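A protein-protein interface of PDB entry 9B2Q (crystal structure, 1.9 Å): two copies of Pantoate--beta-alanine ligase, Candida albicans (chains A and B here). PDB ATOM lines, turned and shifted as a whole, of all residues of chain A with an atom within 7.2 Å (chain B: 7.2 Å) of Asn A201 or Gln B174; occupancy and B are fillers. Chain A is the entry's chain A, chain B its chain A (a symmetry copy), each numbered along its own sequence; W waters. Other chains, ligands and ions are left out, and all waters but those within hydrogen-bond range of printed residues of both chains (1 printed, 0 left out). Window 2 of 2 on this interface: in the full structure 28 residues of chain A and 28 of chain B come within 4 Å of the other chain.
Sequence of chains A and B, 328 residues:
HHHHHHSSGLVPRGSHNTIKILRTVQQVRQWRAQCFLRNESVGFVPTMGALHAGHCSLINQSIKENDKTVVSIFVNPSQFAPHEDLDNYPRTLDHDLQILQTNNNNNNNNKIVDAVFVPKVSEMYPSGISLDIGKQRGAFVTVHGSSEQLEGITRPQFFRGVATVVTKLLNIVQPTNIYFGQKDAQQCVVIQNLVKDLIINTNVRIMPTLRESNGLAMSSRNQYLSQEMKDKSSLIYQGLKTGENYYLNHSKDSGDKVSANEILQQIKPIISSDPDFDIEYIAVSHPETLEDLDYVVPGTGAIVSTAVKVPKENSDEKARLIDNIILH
NE2 of Gln A174 lies close to ND2 of Asn B201, 3.0 Å away.
The backbone carbonyl oxygen (O) of Leu A198 sits close to the side-chain amide oxygen (OD1) of Asn B171, 3.0 Å away.
The backbone carbonyl oxygen (O) of Ile A199 lies within hydrogen-bond range of the guanidinium group (NH2) of Arg B29, 2.7 Å away.
ND2 of Asn A201 lies close to NE2 of Gln B174.
N of Ile A200 sits at hydrogen-bond distance from O of Val A195 (3.0 Å).
The guanidinium group (NH1) of Arg B29 sits at hydrogen-bond distance from the backbone carbonyl oxygen (O) of Asn B171.
The backbone carbonyl oxygen (O) of Ile B172 sits at hydrogen-bond distance from the guanidinium group (NH1) of Arg B29, at 3.3 Å.
NH2 of Arg B32 is in hydrogen-bond range of O of Gln B174.
Leu A198 touches Lys B168.
Ile A199 touches Asn B171.
Ile A199 touches Ile B172 (CG2 to CG1, 3.6 Å).
NH2 of Arg B29 touches C of Ile A200, 3.7 Å away.
Ile A200 touches Asn B171 (CG1 to OD1, 3.7 Å).
N of Asn A201 touches NH2 of Arg B29, at 3.6 Å.
Of the printed residues of chain B, Leu A198 touches Lys B168 (3.8 Å) and Asn B171 (3.0 Å).
Of chain B, only Arg B29 (3.6 Å) and Gln B174 (3.0 Å) come within 4 Å of Asn A201.
Ala B33 touches none of the printed residues of chain A.
Of the printed residues of chain A, Lys B168 touches Leu A198 (3.8 Å).
Of chain A, only Asn A201 (3.0 Å) comes within 4 Å of Gln B174.
Pro B175 touches none of the printed residues of chain A.
Of the printed residues of chain A, Asn B201 touches Gln A174.
The nearest residue of chain B that does not touch Asn A201 is Asn B171 (4.6 Å).
The nearest residue of chain A that does not touch Gln B174 is Gln A174 (4.2 Å).
Of the 13 printed residues of chain A, 5 touch a printed residue of chain B.
Hydrophobic or aromatic side chains of chain A within 4 Å of the printed part of chain B: Leu A198, Ile A199 and Ile A200.
Among the printed residues, no Asp or Glu carboxylate lies within 4 Å of a Lys or Arg side-chain nitrogen of the other chain.
Gln A174 touches Asn B201, and with the chains exchanged Asn A201 touches Gln B174.
Of the 10 pairs that touch across the chains among the printed residues, 2 have their exchanged pair printed and touching as well.
Water W1 lies within hydrogen-bond range of the backbone carbonyl oxygen (O) of Asn B171 (2.8 Å) and the backbone NH (N) of Asn A201 (2.9 Å).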
ATOM      1  N   PHE A  36       9.541  25.457  42.637  1.00  0.00           N
ATOM      2  CA  PHE A  36      10.394  26.017  41.587  1.00  0.00           C
ATOM      3  C   PHE A  36      11.500  26.880  42.194  1.00  0.00           C
ATOM      4  O   PHE A  36      12.676  26.761  41.829  1.00  0.00           O
ATOM      5  CB  PHE A  36       9.571  26.861  40.599  1.00  0.00           C
ATOM      6  CG  PHE A  36       8.883  26.065  39.487  1.00  0.00           C
ATOM      7  CD1 PHE A  36       9.588  25.155  38.711  1.00  0.00           C
ATOM      8  CD2 PHE A  36       7.526  26.258  39.213  1.00  0.00           C
ATOM      9  CE1 PHE A  36       8.940  24.421  37.682  1.00  0.00           C
ATOM     10  CE2 PHE A  36       6.868  25.535  38.186  1.00  0.00           C
ATOM     11  CZ  PHE A  36       7.585  24.618  37.426  1.00  0.00           C
ATOM     12  N   LEU A 170      -1.561  17.474  34.956  1.00  0.00           N
ATOM     13  CA  LEU A 170      -0.157  17.737  34.621  1.00  0.00           C
ATOM     14  C   LEU A 170       0.119  19.229  34.434  1.00  0.00           C
ATOM     15  O   LEU A 170       1.219  19.711  34.764  1.00  0.00           O
ATOM     16  CB  LEU A 170       0.250  16.972  33.360  1.00  0.00           C
ATOM     17  CG  LEU A 170       0.613  15.485  33.484  1.00  0.00           C
ATOM     18  CD1 LEU A 170       0.569  14.816  32.119  1.00  0.00           C
ATOM     19  CD2 LEU A 170       1.998  15.311  34.150  1.00  0.00           C
ATOM     20  N   GLN A 174       2.580  20.462  37.196  1.00  0.00           N
ATOM     21  CA  GLN A 174       3.839  20.544  36.466  1.00  0.00           C
ATOM     22  C   GLN A 174       4.921  19.699  37.139  1.00  0.00           C
ATOM     23  O   GLN A 174       5.952  20.236  37.577  1.00  0.00           O
ATOM     24  CB  GLN A 174       4.279  21.995  36.321  1.00  0.00           C
ATOM     25  CG  GLN A 174       3.208  22.855  35.641  1.00  0.00           C
ATOM     26  CD  GLN A 174       3.712  24.209  35.155  1.00  0.00           C
ATOM     27  OE1 GLN A 174       4.359  24.309  34.107  1.00  0.00           O
ATOM     28  NE2 GLN A 174       3.394  25.256  35.898  1.00  0.00           N
ATOM     29  N   PRO A 175       4.718  18.388  37.264  1.00  0.00           N
ATOM     30  CA  PRO A 175       5.667  17.554  38.005  1.00  0.00           C
ATOM     31  C   PRO A 175       6.863  17.163  37.155  1.00  0.00           C
ATOM     32  O   PRO A 175       6.817  17.159  35.921  1.00  0.00           O
ATOM     33  CB  PRO A 175       4.844  16.313  38.370  1.00  0.00           C
ATOM     34  CG  PRO A 175       3.898  16.167  37.187  1.00  0.00           C
ATOM     35  CD  PRO A 175       3.612  17.587  36.694  1.00  0.00           C
ATOM     36  N   THR A 176       7.947  16.837  37.866  1.00  0.00           N
ATOM     37  CA  THR A 176       9.107  16.197  37.256  1.00  0.00           C
ATOM     38  C   THR A 176       8.794  14.764  36.851  1.00  0.00           C
ATOM     39  O   THR A 176       9.242  14.291  35.800  1.00  0.00           O
ATOM     40  CB  THR A 176      10.282  16.211  38.247  1.00  0.00           C
ATOM     41  OG1 THR A 176      10.385  17.507  38.861  1.00  0.00           O
ATOM     42  CG2 THR A 176      11.592  15.859  37.541  1.00  0.00           C
ATOM     43  N   ASN A 177       8.033  14.060  37.681  1.00  0.00           N
ATOM     44  CA  ASN A 177       7.687  12.659  37.486  1.00  0.00           C
ATOM     45  C   ASN A 177       6.229  12.466  37.866  1.00  0.00           C
ATOM     46  O   ASN A 177       5.766  13.064  38.844  1.00  0.00           O
ATOM     47  CB  ASN A 177       8.562  11.743  38.358  1.00  0.00           C
ATOM     48  CG  ASN A 177      10.039  11.805  37.986  1.00  0.00           C
ATOM     49  OD1 ASN A 177      10.442  11.270  36.960  1.00  0.00           O
ATOM     50  ND2 ASN A 177      10.852  12.423  38.839  1.00  0.00           N
ATOM     51  N   VAL A 195       1.762  11.771  26.889  1.00  0.00           N
ATOM     52  CA  VAL A 195       2.953  12.570  27.175  1.00  0.00           C
ATOM     53  C   VAL A 195       3.874  12.616  25.957  1.00  0.00           C
ATOM     54  O   VAL A 195       4.464  13.659  25.644  1.00  0.00           O
ATOM     55  CB  VAL A 195       3.647  12.005  28.425  1.00  0.00           C
ATOM     56  CG1 VAL A 195       5.057  12.631  28.631  1.00  0.00           C
ATOM     57  CG2 VAL A 195       2.758  12.264  29.638  1.00  0.00           C
ATOM     58  N   LEU A 198       1.673  14.902  23.123  1.00  0.00           N
ATOM     59  CA  LEU A 198       1.557  16.308  23.479  1.00  0.00           C
ATOM     60  C   LEU A 198       2.899  16.896  23.901  1.00  0.00           C
ATOM     61  O   LEU A 198       2.972  18.092  24.208  1.00  0.00           O
ATOM     62  CB  LEU A 198       0.502  16.508  24.582  1.00  0.00           C
ATOM     63  CG  LEU A 198      -0.950  16.166  24.157  1.00  0.00           C
ATOM     64  CD1 LEU A 198      -1.931  16.564  25.270  1.00  0.00           C
ATOM     65  CD2 LEU A 198      -1.348  16.837  22.833  1.00  0.00           C
ATOM     66  N   ILE A 199       3.956  16.078  23.882  1.00  0.00           N
ATOM     67  CA  ILE A 199       5.346  16.494  24.053  1.00  0.00           C
ATOM     68  C   ILE A 199       5.509  17.173  25.415  1.00  0.00           C
ATOM     69  O   ILE A 199       6.132  18.236  25.544  1.00  0.00           O
ATOM     70  CB  ILE A 199       5.806  17.363  22.865  1.00  0.00           C
ATOM     71  CG1 ILE A 199       5.262  16.736  21.547  1.00  0.00           C
ATOM     72  CG2 ILE A 199       7.307  17.397  22.812  1.00  0.00           C
ATOM     73  CD1 ILE A 199       5.693  17.437  20.253  1.00  0.00           C
ATOM     74  N   ILE A 200       5.004  16.511  26.462  1.00  0.00           N
ATOM     75  CA  ILE A 200       4.965  17.063  27.817  1.00  0.00           C
ATOM     76  C   ILE A 200       6.287  16.806  28.535  1.00  0.00           C
ATOM     77  O   ILE A 200       6.821  15.693  28.506  1.00  0.00           O
ATOM     78  CB  ILE A 200       3.777  16.455  28.594  1.00  0.00           C
ATOM     79  CG1 ILE A 200       2.452  16.697  27.843  1.00  0.00           C
ATOM     80  CG2 ILE A 200       3.711  16.992  30.029  1.00  0.00           C
ATOM     81  CD1 ILE A 200       1.221  16.069  28.522  1.00  0.00           C
ATOM     82  N   ASN A 201       6.792  17.834  29.234  1.00  0.00           N
ATOM     83  CA  ASN A 201       8.084  17.783  29.931  1.00  0.00           C
ATOM     84  C   ASN A 201       7.964  17.151  31.329  1.00  0.00           C
ATOM     85  O   ASN A 201       8.221  17.790  32.352  1.00  0.00           O
ATOM     86  CB  ASN A 201       8.677  19.191  30.024  1.00  0.00           C
ATOM     87  CG  ASN A 201      10.134  19.192  30.483  1.00  0.00           C
ATOM     88  OD1 ASN A 201      10.800  18.154  30.466  1.00  0.00           O
ATOM     89  ND2 ASN A 201      10.641  20.365  30.882  1.00  0.00           N
ATOM     90  N   THR A 202       7.599  15.866  31.349  1.00  0.00           N
ATOM     91  CA  THR A 202       7.501  15.059  32.564  1.00  0.00           C
ATOM     92  C   THR A 202       7.901  13.621  32.228  1.00  0.00           C
ATOM     93  O   THR A 202       7.712  13.167  31.093  1.00  0.00           O
ATOM     94  CB  THR A 202       6.066  15.097  33.129  1.00  0.00           C
ATOM     95  OG1 THR A 202       5.654  16.453  33.342  1.00  0.00           O
ATOM     96  CG2 THR A 202       5.946  14.337  34.444  1.00  0.00           C
ATOM     97  N   ASN A 203       8.452  12.900  33.210  1.00  0.00           N
ATOM     98  CA  ASN A 203       8.668  11.459  33.073  1.00  0.00           C
ATOM     99  C   ASN A 203       7.437  10.700  33.568  1.00  0.00           C
ATOM    100  O   ASN A 203       6.947  10.962  34.670  1.00  0.00           O
ATOM    101  CB  ASN A 203       9.893  10.989  33.860  1.00  0.00           C
ATOM    102  CG  ASN A 203      11.157  11.747  33.503  1.00  0.00           C
ATOM    103  OD1 ASN A 203      11.451  11.962  32.326  1.00  0.00           O
ATOM    104  ND2 ASN A 203      11.920  12.159  34.529  1.00  0.00           N
ATOM    105  N   GLN B  26      14.517  18.621  21.710  1.00  0.00           N
ATOM    106  CA  GLN B  26      15.540  18.608  22.752  1.00  0.00           C
ATOM    107  C   GLN B  26      16.379  19.877  22.727  1.00  0.00           C
ATOM    108  O   GLN B  26      16.774  20.382  23.784  1.00  0.00           O
ATOM    109  CB  GLN B  26      16.422  17.369  22.618  1.00  0.00           C
ATOM    110  CG  GLN B  26      15.721  16.097  23.129  1.00  0.00           C
ATOM    111  CD  GLN B  26      15.071  16.278  24.507  1.00  0.00           C
ATOM    112  OE1 GLN B  26      13.862  16.067  24.668  1.00  0.00           O
ATOM    113  NE2 GLN B  26      15.869  16.657  25.503  1.00  0.00           N
ATOM    114  N   VAL B  28      15.209  22.819  21.903  1.00  0.00           N
ATOM    115  CA  VAL B  28      14.379  23.812  22.582  1.00  0.00           C
ATOM    116  C   VAL B  28      14.374  23.558  24.083  1.00  0.00           C
ATOM    117  O   VAL B  28      14.423  24.503  24.880  1.00  0.00           O
ATOM    118  CB  VAL B  28      12.938  23.823  22.029  1.00  0.00           C
ATOM    119  CG1 VAL B  28      12.113  24.888  22.752  1.00  0.00           C
ATOM    120  CG2 VAL B  28      12.918  24.075  20.530  1.00  0.00           C
ATOM    121  N   ARG B  29      14.285  22.290  24.498  1.00  0.00           N
ATOM    122  CA  ARG B  29      14.328  21.996  25.931  1.00  0.00           C
ATOM    123  C   ARG B  29      15.603  22.550  26.562  1.00  0.00           C
ATOM    124  O   ARG B  29      15.564  23.156  27.639  1.00  0.00           O
ATOM    125  CB  ARG B  29      14.252  20.492  26.172  1.00  0.00           C
ATOM    126  CG  ARG B  29      12.920  19.874  25.826  1.00  0.00           C
ATOM    127  CD  ARG B  29      12.172  19.454  27.073  1.00  0.00           C
ATOM    128  NE  ARG B  29      10.947  18.745  26.716  1.00  0.00           N
ATOM    129  CZ  ARG B  29       9.758  19.316  26.602  1.00  0.00           C
ATOM    130  NH1 ARG B  29       9.597  20.620  26.777  1.00  0.00           N
ATOM    131  NH2 ARG B  29       8.705  18.559  26.312  1.00  0.00           N
ATOM    132  N   ARG B  32      15.364  26.357  26.582  1.00  0.00           N
ATOM    133  CA  ARG B  32      14.412  26.779  27.613  1.00  0.00           C
ATOM    134  C   ARG B  32      14.929  26.477  29.016  1.00  0.00           C
ATOM    135  O   ARG B  32      14.625  27.215  29.966  1.00  0.00           O
ATOM    136  CB  ARG B  32      13.054  26.099  27.391  1.00  0.00           C
ATOM    137  CG  ARG B  32      11.937  26.533  28.370  1.00  0.00           C
ATOM    138  CD  ARG B  32      11.539  27.986  28.133  1.00  0.00           C
ATOM    139  NE  ARG B  32      10.489  28.439  29.041  1.00  0.00           N
ATOM    140  CZ  ARG B  32      10.698  28.931  30.258  1.00  0.00           C
ATOM    141  NH1 ARG B  32      11.916  29.004  30.778  1.00  0.00           N
ATOM    142  NH2 ARG B  32       9.663  29.369  30.969  1.00  0.00           N
ATOM    143  N   ALA B  33      15.703  25.402  29.176  1.00  0.00           N
ATOM    144  CA  ALA B  33      16.240  25.096  30.496  1.00  0.00           C
ATOM    145  C   ALA B  33      17.255  26.146  30.930  1.00  0.00           C
ATOM    146  O   ALA B  33      17.381  26.436  32.128  1.00  0.00           O
ATOM    147  CB  ALA B  33      16.873  23.707  30.505  1.00  0.00           C
ATOM    148  N   PHE B  36      15.214  28.954  32.172  1.00  0.00           N
ATOM    149  CA  PHE B  36      14.800  28.624  33.538  1.00  0.00           C
ATOM    150  C   PHE B  36      15.925  28.925  34.529  1.00  0.00           C
ATOM    151  O   PHE B  36      15.703  29.543  35.578  1.00  0.00           O
ATOM    152  CB  PHE B  36      14.403  27.141  33.651  1.00  0.00           C
ATOM    153  CG  PHE B  36      12.963  26.826  33.238  1.00  0.00           C
ATOM    154  CD1 PHE B  36      11.892  27.545  33.753  1.00  0.00           C
ATOM    155  CD2 PHE B  36      12.694  25.784  32.346  1.00  0.00           C
ATOM    156  CE1 PHE B  36      10.561  27.245  33.363  1.00  0.00           C
ATOM    157  CE2 PHE B  36      11.368  25.470  31.953  1.00  0.00           C
ATOM    158  CZ  PHE B  36      10.308  26.208  32.466  1.00  0.00           C
ATOM    159  N   VAL B  42       9.782  34.260  29.261  1.00  0.00           N
ATOM    160  CA  VAL B  42       9.895  33.769  27.894  1.00  0.00           C
ATOM    161  C   VAL B  42       8.596  34.084  27.155  1.00  0.00           C
ATOM    162  O   VAL B  42       7.521  33.591  27.535  1.00  0.00           O
ATOM    163  CB  VAL B  42      10.191  32.258  27.852  1.00  0.00           C
ATOM    164  CG1 VAL B  42      10.117  31.734  26.431  1.00  0.00           C
ATOM    165  CG2 VAL B  42      11.556  31.938  28.497  1.00  0.00           C
ATOM    166  N   PHE B  44       6.524  33.963  23.412  1.00  0.00           N
ATOM    167  CA  PHE B  44       6.467  32.974  22.333  1.00  0.00           C
ATOM    168  C   PHE B  44       5.489  33.432  21.256  1.00  0.00           C
ATOM    169  O   PHE B  44       4.327  33.714  21.559  1.00  0.00           O
ATOM    170  CB  PHE B  44       6.043  31.604  22.894  1.00  0.00           C
ATOM    171  CG  PHE B  44       5.826  30.532  21.848  1.00  0.00           C
ATOM    172  CD1 PHE B  44       6.694  30.391  20.781  1.00  0.00           C
ATOM    173  CD2 PHE B  44       4.770  29.628  21.976  1.00  0.00           C
ATOM    174  CE1 PHE B  44       6.490  29.391  19.823  1.00  0.00           C
ATOM    175  CE2 PHE B  44       4.559  28.632  21.027  1.00  0.00           C
ATOM    176  CZ  PHE B  44       5.427  28.502  19.959  1.00  0.00           C
ATOM    177  N   LYS B 168       0.894  21.252  21.732  1.00  0.00           N
ATOM    178  CA  LYS B 168       2.252  20.712  21.621  1.00  0.00           C
ATOM    179  C   LYS B 168       3.306  21.811  21.765  1.00  0.00           C
ATOM    180  O   LYS B 168       4.297  21.645  22.486  1.00  0.00           O
ATOM    181  CB  LYS B 168       2.418  19.988  20.276  1.00  0.00           C
ATOM    182  CG  LYS B 168       1.576  18.671  20.130  1.00  0.00           C
ATOM    183  CD  LYS B 168       1.449  18.329  18.620  1.00  0.00           C
ATOM    184  CE  LYS B 168       0.639  17.049  18.353  1.00  0.00           C
ATOM    185  NZ  LYS B 168       1.475  15.788  18.355  1.00  0.00           N
ATOM    186  N   LEU B 169       3.135  22.925  21.035  1.00  0.00           N
ATOM    187  CA  LEU B 169       4.105  24.024  21.104  1.00  0.00           C
ATOM    188  C   LEU B 169       4.202  24.597  22.512  1.00  0.00           C
ATOM    189  O   LEU B 169       5.305  24.906  22.994  1.00  0.00           O
ATOM    190  CB  LEU B 169       3.702  25.118  20.110  1.00  0.00           C
ATOM    191  CG  LEU B 169       3.864  24.670  18.652  1.00  0.00           C
ATOM    192  CD1 LEU B 169       3.086  25.597  17.692  1.00  0.00           C
ATOM    193  CD2 LEU B 169       5.348  24.596  18.283  1.00  0.00           C
ATOM    194  N   LEU B 170       3.055  24.785  23.185  1.00  0.00           N
ATOM    195  CA  LEU B 170       3.108  25.284  24.564  1.00  0.00           C
ATOM    196  C   LEU B 170       3.863  24.331  25.490  1.00  0.00           C
ATOM    197  O   LEU B 170       4.541  24.777  26.434  1.00  0.00           O
ATOM    198  CB  LEU B 170       1.697  25.524  25.106  1.00  0.00           C
ATOM    199  CG  LEU B 170       0.971  26.821  24.721  1.00  0.00           C
ATOM    200  CD1 LEU B 170      -0.521  26.689  24.986  1.00  0.00           C
ATOM    201  CD2 LEU B 170       1.568  28.031  25.476  1.00  0.00           C
ATOM    202  N   ASN B 171       3.757  23.020  25.247  1.00  0.00           N
ATOM    203  CA  ASN B 171       4.462  22.042  26.079  1.00  0.00           C
ATOM    204  C   ASN B 171       5.957  21.973  25.766  1.00  0.00           C
ATOM    205  O   ASN B 171       6.748  21.589  26.640  1.00  0.00           O
ATOM    206  CB  ASN B 171       3.825  20.656  25.912  1.00  0.00           C
ATOM    207  CG  ASN B 171       2.502  20.525  26.651  1.00  0.00           C
ATOM    208  OD1 ASN B 171       1.533  19.889  26.178  1.00  0.00           O
ATOM    209  ND2 ASN B 171       2.455  21.111  27.815  1.00  0.00           N
ATOM    210  N   ILE B 172       6.353  22.309  24.529  1.00  0.00           N
ATOM    211  CA  ILE B 172       7.772  22.365  24.165  1.00  0.00           C
ATOM    212  C   ILE B 172       8.422  23.631  24.719  1.00  0.00           C
ATOM    213  O   ILE B 172       9.468  23.583  25.391  1.00  0.00           O
ATOM    214  CB  ILE B 172       7.930  22.287  22.622  1.00  0.00           C
ATOM    215  CG1 ILE B 172       7.452  20.942  22.075  1.00  0.00           C
ATOM    216  CG2 ILE B 172       9.394  22.566  22.207  1.00  0.00           C
ATOM    217  CD1 ILE B 172       7.243  20.938  20.514  1.00  0.00           C
ATOM    218  N   VAL B 173       7.813  24.789  24.444  1.00  0.00           N
ATOM    219  CA  VAL B 173       8.435  26.080  24.770  1.00  0.00           C
ATOM    220  C   VAL B 173       8.217  26.473  26.229  1.00  0.00           C
ATOM    221  O   VAL B 173       9.082  27.134  26.843  1.00  0.00           O
ATOM    222  CB  VAL B 173       7.897  27.156  23.806  1.00  0.00           C
ATOM    223  CG1 VAL B 173       8.428  28.552  24.206  1.00  0.00           C
ATOM    224  CG2 VAL B 173       8.334  26.814  22.380  1.00  0.00           C
ATOM    225  N   GLN B 174       7.094  26.071  26.807  1.00  0.00           N
ATOM    226  CA  GLN B 174       6.707  26.445  28.162  1.00  0.00           C
ATOM    227  C   GLN B 174       6.882  27.947  28.390  1.00  0.00           C
ATOM    228  O   GLN B 174       7.671  28.360  29.256  1.00  0.00           O
ATOM    229  CB  GLN B 174       7.492  25.633  29.184  1.00  0.00           C
ATOM    230  CG  GLN B 174       7.322  24.125  28.975  1.00  0.00           C
ATOM    231  CD  GLN B 174       7.784  23.275  30.153  1.00  0.00           C
ATOM    232  OE1 GLN B 174       7.079  23.145  31.160  1.00  0.00           O
ATOM    233  NE2 GLN B 174       8.954  22.674  30.021  1.00  0.00           N
ATOM    234  N   PRO B 175       6.192  28.791  27.624  1.00  0.00           N
ATOM    235  CA  PRO B 175       6.412  30.235  27.721  1.00  0.00           C
ATOM    236  C   PRO B 175       5.644  30.850  28.878  1.00  0.00           C
ATOM    237  O   PRO B 175       4.647  30.309  29.364  1.00  0.00           O
ATOM    238  CB  PRO B 175       5.881  30.768  26.386  1.00  0.00           C
ATOM    239  CG  PRO B 175       4.733  29.821  26.068  1.00  0.00           C
ATOM    240  CD  PRO B 175       5.133  28.460  26.643  1.00  0.00           C
ATOM    241  N   THR B 176       6.153  32.008  29.309  1.00  0.00           N
ATOM    242  CA  THR B 176       5.429  32.876  30.230  1.00  0.00           C
ATOM    243  C   THR B 176       4.228  33.518  29.551  1.00  0.00           C
ATOM    244  O   THR B 176       3.162  33.667  30.159  1.00  0.00           O
ATOM    245  CB  THR B 176       6.373  33.968  30.758  1.00  0.00           C
ATOM    246  OG1 THR B 176       7.635  33.385  31.123  1.00  0.00           O
ATOM    247  CG2 THR B 176       5.757  34.683  31.962  1.00  0.00           C
ATOM    248  N   ASN B 177       4.392  33.910  28.293  1.00  0.00           N
ATOM    249  CA  ASN B 177       3.374  34.598  27.511  1.00  0.00           C
ATOM    250  C   ASN B 177       3.392  34.039  26.098  1.00  0.00           C
ATOM    251  O   ASN B 177       4.471  33.763  25.562  1.00  0.00           O
ATOM    252  CB  ASN B 177       3.643  36.112  27.458  1.00  0.00           C
ATOM    253  CG  ASN B 177       3.557  36.777  28.827  1.00  0.00           C
ATOM    254  OD1 ASN B 177       2.469  36.953  29.362  1.00  0.00           O
ATOM    255  ND2 ASN B 177       4.700  37.181  29.376  1.00  0.00           N
ATOM    256  N   ASN B 201      -0.327  27.023  32.469  1.00  0.00           N
ATOM    257  CA  ASN B 201       0.358  28.105  33.188  1.00  0.00           C
ATOM    258  C   ASN B 201       1.095  29.060  32.233  1.00  0.00           C
ATOM    259  O   ASN B 201       2.320  29.196  32.272  1.00  0.00           O
ATOM    260  CB  ASN B 201       1.326  27.514  34.214  1.00  0.00           C
ATOM    261  CG  ASN B 201       1.869  28.557  35.189  1.00  0.00           C
ATOM    262  OD1 ASN B 201       1.328  29.660  35.296  1.00  0.00           O
ATOM    263  ND2 ASN B 201       2.936  28.206  35.917  1.00  0.00           N
ATOM    264  N   THR B 202       0.316  29.748  31.393  1.00  0.00           N
ATOM    265  CA  THR B 202       0.807  30.760  30.460  1.00  0.00           C
ATOM    266  C   THR B 202      -0.256  31.852  30.321  1.00  0.00           C
ATOM    267  O   THR B 202      -1.454  31.581  30.462  1.00  0.00           O
ATOM    268  CB  THR B 202       1.111  30.131  29.084  1.00  0.00           C
ATOM    269  OG1 THR B 202       2.026  29.037  29.232  1.00  0.00           O
ATOM    270  CG2 THR B 202       1.706  31.140  28.111  1.00  0.00           C
HETATM  271  O   HOH W   1       5.645  20.466  28.926  1.00  0.00           O
